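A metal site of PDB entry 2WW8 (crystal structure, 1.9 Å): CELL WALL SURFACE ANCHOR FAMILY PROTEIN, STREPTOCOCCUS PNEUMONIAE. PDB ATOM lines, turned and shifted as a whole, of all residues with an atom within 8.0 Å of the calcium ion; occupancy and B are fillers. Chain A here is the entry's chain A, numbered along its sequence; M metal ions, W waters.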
ATOM      1  N   LEU A 363     -23.675  20.378  32.925  1.00  0.00           N
ATOM      2  CA  LEU A 363     -23.563  20.498  31.459  1.00  0.00           C
ATOM      3  C   LEU A 363     -22.318  19.715  31.003  1.00  0.00           C
ATOM      4  O   LEU A 363     -22.362  19.021  29.993  1.00  0.00           O
ATOM      5  CB  LEU A 363     -23.455  21.996  31.094  1.00  0.00           C
ATOM      6  CG  LEU A 363     -24.750  22.798  31.217  1.00  0.00           C
ATOM      7  CD1 LEU A 363     -24.420  24.324  31.123  1.00  0.00           C
ATOM      8  CD2 LEU A 363     -25.852  22.375  30.222  1.00  0.00           C
ATOM      9  N   MET A 364     -21.207  19.822  31.736  1.00  0.00           N
ATOM     10  CA  MET A 364     -20.041  19.006  31.451  1.00  0.00           C
ATOM     11  C   MET A 364     -20.244  17.509  31.427  1.00  0.00           C
ATOM     12  O   MET A 364     -19.732  16.839  30.518  1.00  0.00           O
ATOM     13  CB  MET A 364     -18.807  19.331  32.319  1.00  0.00           C
ATOM     14  CG  MET A 364     -18.302  20.719  32.103  1.00  0.00           C
ATOM     15  SD  MET A 364     -17.243  21.312  33.443  1.00  0.00           S
ATOM     16  CE  MET A 364     -15.983  19.959  33.554  1.00  0.00           C
ATOM     17  N   ALA A 366     -23.194  15.999  30.887  1.00  0.00           N
ATOM     18  CA  ALA A 366     -23.994  15.668  29.695  1.00  0.00           C
ATOM     19  C   ALA A 366     -23.114  15.654  28.428  1.00  0.00           C
ATOM     20  O   ALA A 366     -23.178  14.725  27.632  1.00  0.00           O
ATOM     21  CB  ALA A 366     -25.131  16.659  29.478  1.00  0.00           C
ATOM     22  N   ASP A 367     -22.248  16.644  28.239  1.00  0.00           N
ATOM     23  CA  ASP A 367     -21.359  16.629  27.057  1.00  0.00           C
ATOM     24  C   ASP A 367     -20.423  15.398  27.073  1.00  0.00           C
ATOM     25  O   ASP A 367     -20.241  14.775  26.035  1.00  0.00           O
ATOM     26  CB  ASP A 367     -20.513  17.911  27.090  1.00  0.00           C
ATOM     27  CG  ASP A 367     -19.749  18.149  25.811  1.00  0.00           C
ATOM     28  OD1 ASP A 367     -20.214  17.799  24.731  1.00  0.00           O
ATOM     29  OD2 ASP A 367     -18.661  18.748  25.851  1.00  0.00           O
ATOM     30  N   GLU A 368     -19.894  15.023  28.244  1.00  0.00           N
ATOM     31  CA  GLU A 368     -19.064  13.821  28.377  1.00  0.00           C
ATOM     32  C   GLU A 368     -19.801  12.537  27.973  1.00  0.00           C
ATOM     33  O   GLU A 368     -19.288  11.737  27.171  1.00  0.00           O
ATOM     34  CB  GLU A 368     -18.524  13.686  29.823  1.00  0.00           C
ATOM     35  CG  GLU A 368     -17.767  12.419  30.115  1.00  0.00           C
ATOM     36  CD  GLU A 368     -17.156  12.441  31.542  1.00  0.00           C
ATOM     37  OE1 GLU A 368     -17.524  13.223  32.450  1.00  0.00           O
ATOM     38  OE2 GLU A 368     -16.215  11.671  31.759  1.00  0.00           O
ATOM     39  N   LEU A 370     -22.547  12.182  26.047  1.00  0.00           N
ATOM     40  CA  LEU A 370     -22.841  12.188  24.586  1.00  0.00           C
ATOM     41  C   LEU A 370     -21.562  12.040  23.764  1.00  0.00           C
ATOM     42  O   LEU A 370     -21.522  11.235  22.827  1.00  0.00           O
ATOM     43  CB  LEU A 370     -23.574  13.477  24.267  1.00  0.00           C
ATOM     44  CG  LEU A 370     -24.998  13.535  24.793  1.00  0.00           C
ATOM     45  CD1 LEU A 370     -25.483  14.968  24.650  1.00  0.00           C
ATOM     46  CD2 LEU A 370     -25.941  12.495  24.008  1.00  0.00           C
ATOM     47  N   THR A 371     -20.495  12.743  24.161  1.00  0.00           N
ATOM     48  CA  THR A 371     -19.241  12.603  23.435  1.00  0.00           C
ATOM     49  C   THR A 371     -18.745  11.143  23.465  1.00  0.00           C
ATOM     50  O   THR A 371     -18.292  10.567  22.467  1.00  0.00           O
ATOM     51  CB  THR A 371     -18.191  13.656  23.947  1.00  0.00           C
ATOM     52  OG1 THR A 371     -18.680  14.977  23.653  1.00  0.00           O
ATOM     53  CG2 THR A 371     -16.870  13.452  23.163  1.00  0.00           C
ATOM     54  N   LEU A 426     -12.828  24.059  27.348  1.00  0.00           N
ATOM     55  CA  LEU A 426     -12.738  23.461  28.675  1.00  0.00           C
ATOM     56  C   LEU A 426     -11.300  23.419  29.227  1.00  0.00           C
ATOM     57  O   LEU A 426     -11.084  23.585  30.444  1.00  0.00           O
ATOM     58  CB  LEU A 426     -13.344  22.038  28.692  1.00  0.00           C
ATOM     59  CG  LEU A 426     -13.558  21.370  30.064  1.00  0.00           C
ATOM     60  CD1 LEU A 426     -14.346  22.188  31.077  1.00  0.00           C
ATOM     61  CD2 LEU A 426     -14.151  19.944  29.843  1.00  0.00           C
ATOM     62  N   TYR A 522     -18.457  28.703  28.863  1.00  0.00           N
ATOM     63  CA  TYR A 522     -18.215  27.263  28.857  1.00  0.00           C
ATOM     64  C   TYR A 522     -19.137  26.614  27.785  1.00  0.00           C
ATOM     65  O   TYR A 522     -18.718  25.806  26.924  1.00  0.00           O
ATOM     66  CB  TYR A 522     -18.415  26.568  30.208  1.00  0.00           C
ATOM     67  CG  TYR A 522     -18.632  25.060  29.929  1.00  0.00           C
ATOM     68  CD1 TYR A 522     -17.594  24.208  29.541  1.00  0.00           C
ATOM     69  CD2 TYR A 522     -19.921  24.544  29.941  1.00  0.00           C
ATOM     70  CE1 TYR A 522     -17.862  22.863  29.236  1.00  0.00           C
ATOM     71  CE2 TYR A 522     -20.210  23.204  29.631  1.00  0.00           C
ATOM     72  CZ  TYR A 522     -19.141  22.394  29.306  1.00  0.00           C
ATOM     73  OH  TYR A 522     -19.387  21.092  28.966  1.00  0.00           O
ATOM     74  N   TYR A 523     -20.423  26.951  27.849  1.00  0.00           N
ATOM     75  CA  TYR A 523     -21.441  26.378  26.953  1.00  0.00           C
ATOM     76  C   TYR A 523     -21.104  26.707  25.494  1.00  0.00           C
ATOM     77  O   TYR A 523     -21.044  25.796  24.645  1.00  0.00           O
ATOM     78  CB  TYR A 523     -22.846  26.895  27.313  1.00  0.00           C
ATOM     79  CG  TYR A 523     -23.940  26.292  26.458  1.00  0.00           C
ATOM     80  CD1 TYR A 523     -24.270  26.830  25.209  1.00  0.00           C
ATOM     81  CD2 TYR A 523     -24.650  25.177  26.899  1.00  0.00           C
ATOM     82  CE1 TYR A 523     -25.307  26.271  24.386  1.00  0.00           C
ATOM     83  CE2 TYR A 523     -25.683  24.645  26.136  1.00  0.00           C
ATOM     84  CZ  TYR A 523     -25.983  25.178  24.899  1.00  0.00           C
ATOM     85  OH  TYR A 523     -26.983  24.551  24.178  1.00  0.00           O
ATOM     86  N   GLY A 525     -18.336  27.542  24.229  1.00  0.00           N
ATOM     87  CA  GLY A 525     -17.062  26.970  23.783  1.00  0.00           C
ATOM     88  C   GLY A 525     -17.042  25.456  23.547  1.00  0.00           C
ATOM     89  O   GLY A 525     -16.256  24.977  22.742  1.00  0.00           O
ATOM     90  N   ASN A 526     -17.894  24.717  24.245  1.00  0.00           N
ATOM     91  CA  ASN A 526     -17.760  23.242  24.334  1.00  0.00           C
ATOM     92  C   ASN A 526     -19.033  22.462  24.100  1.00  0.00           C
ATOM     93  O   ASN A 526     -18.988  21.217  23.983  1.00  0.00           O
ATOM     94  CB  ASN A 526     -17.295  22.886  25.777  1.00  0.00           C
ATOM     95  CG  ASN A 526     -15.969  23.573  26.107  1.00  0.00           C
ATOM     96  OD1 ASN A 526     -14.913  23.162  25.649  1.00  0.00           O
ATOM     97  ND2 ASN A 526     -16.080  24.726  26.737  1.00  0.00           N
ATOM     98  N   ILE A 527     -20.168  23.151  24.108  1.00  0.00           N
ATOM     99  CA  ILE A 527     -21.419  22.468  23.861  1.00  0.00           C
ATOM    100  C   ILE A 527     -22.097  22.967  22.588  1.00  0.00           C
ATOM    101  O   ILE A 527     -22.492  22.191  21.758  1.00  0.00           O
ATOM    102  CB  ILE A 527     -22.358  22.579  25.053  1.00  0.00           C
ATOM    103  CG1 ILE A 527     -21.780  21.759  26.229  1.00  0.00           C
ATOM    104  CG2 ILE A 527     -23.777  21.978  24.674  1.00  0.00           C
ATOM    105  CD1 ILE A 527     -22.712  21.620  27.347  1.00  0.00           C
ATOM    106  N   ALA A 528     -22.218  24.283  22.413  1.00  0.00           N
ATOM    107  CA  ALA A 528     -22.840  24.885  21.229  1.00  0.00           C
ATOM    108  C   ALA A 528     -22.291  24.374  19.869  1.00  0.00           C
ATOM    109  O   ALA A 528     -23.079  24.161  18.964  1.00  0.00           O
ATOM    110  CB  ALA A 528     -22.717  26.403  21.276  1.00  0.00           C
ATOM    111  N   PRO A 529     -20.971  24.152  19.717  1.00  0.00           N
ATOM    112  CA  PRO A 529     -20.464  23.695  18.385  1.00  0.00           C
ATOM    113  C   PRO A 529     -20.839  22.247  18.055  1.00  0.00           C
ATOM    114  O   PRO A 529     -20.701  21.841  16.942  1.00  0.00           O
ATOM    115  CB  PRO A 529     -18.926  23.776  18.547  1.00  0.00           C
ATOM    116  CG  PRO A 529     -18.729  24.652  19.791  1.00  0.00           C
ATOM    117  CD  PRO A 529     -19.899  24.363  20.703  1.00  0.00           C
ATOM    118  N   ASP A 530     -21.342  21.463  19.001  1.00  0.00           N
ATOM    119  CA  ASP A 530     -21.714  20.079  18.771  1.00  0.00           C
ATOM    120  C   ASP A 530     -23.080  19.783  18.131  1.00  0.00           C
ATOM    121  O   ASP A 530     -23.304  18.655  17.741  1.00  0.00           O
ATOM    122  CB  ASP A 530     -21.625  19.326  20.093  1.00  0.00           C
ATOM    123  CG  ASP A 530     -20.203  19.409  20.698  1.00  0.00           C
ATOM    124  OD1 ASP A 530     -19.220  19.693  19.982  1.00  0.00           O
ATOM    125  OD2 ASP A 530     -20.073  19.157  21.898  1.00  0.00           O
ATOM    126  N   TYR A 532     -26.093  19.612  19.313  1.00  0.00           N
ATOM    127  CA  TYR A 532     -27.106  19.014  20.180  1.00  0.00           C
ATOM    128  C   TYR A 532     -28.395  19.805  20.154  1.00  0.00           C
ATOM    129  O   TYR A 532     -28.368  21.038  19.991  1.00  0.00           O
ATOM    130  CB  TYR A 532     -26.650  18.905  21.604  1.00  0.00           C
ATOM    131  CG  TYR A 532     -25.359  18.207  21.943  1.00  0.00           C
ATOM    132  CD1 TYR A 532     -24.856  17.164  21.168  1.00  0.00           C
ATOM    133  CD2 TYR A 532     -24.600  18.648  23.043  1.00  0.00           C
ATOM    134  CE1 TYR A 532     -23.619  16.519  21.501  1.00  0.00           C
ATOM    135  CE2 TYR A 532     -23.417  18.055  23.369  1.00  0.00           C
ATOM    136  CZ  TYR A 532     -22.959  16.965  22.626  1.00  0.00           C
ATOM    137  OH  TYR A 532     -21.763  16.360  22.966  1.00  0.00           O
HETATM  138 CA    CA M   1     -18.329  19.114  23.501  1.00  0.00          CA
HETATM  139  O   HOH W   1     -17.485  17.015  22.653  1.00  0.00           O
HETATM  140  O   HOH W   2     -16.131  19.688  24.210  1.00  0.00           O
HETATM  141  O   HOH W   3     -17.177  20.188  21.628  1.00  0.00           O
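The side-chain hydroxyl (OH) of Tyr 532 sits close to the side-chain carboxylate (OD2) of Asp 530 (3.4 Å).
The backbone carbonyl oxygen of Tyr 522 is in hydrogen-bond range of the side-chain amide nitrogen of Asn 526, 2.9 Å away.
The side-chain hydroxyl (OG1) of Thr 371 lies within hydrogen-bond range of the backbone carbonyl oxygen (O) of Asp 367 (2.9 Å).
The side-chain amide oxygen of Asn 526 is in hydrogen-bond range of the backbone NH of Leu 426 (2.8 Å).
The side-chain carboxylate of Asp 367 lies close to the side-chain hydroxyl of Tyr 532 (2.8 Å).
Of the 17 residues printed, 3 come within 4 Å of the calcium ion.
The calcium ion is bound by the backbone carbonyl oxygen (O) of Asn 526, the side-chain carboxylate (OD2) of Asp 530, water W2, the side-chain carboxylate (OD2) of Asp 367, water W1, water W3 and the side-chain carboxylate (OD1) of Asp 367.
The calcium ion has seven donor atoms within binding distance.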
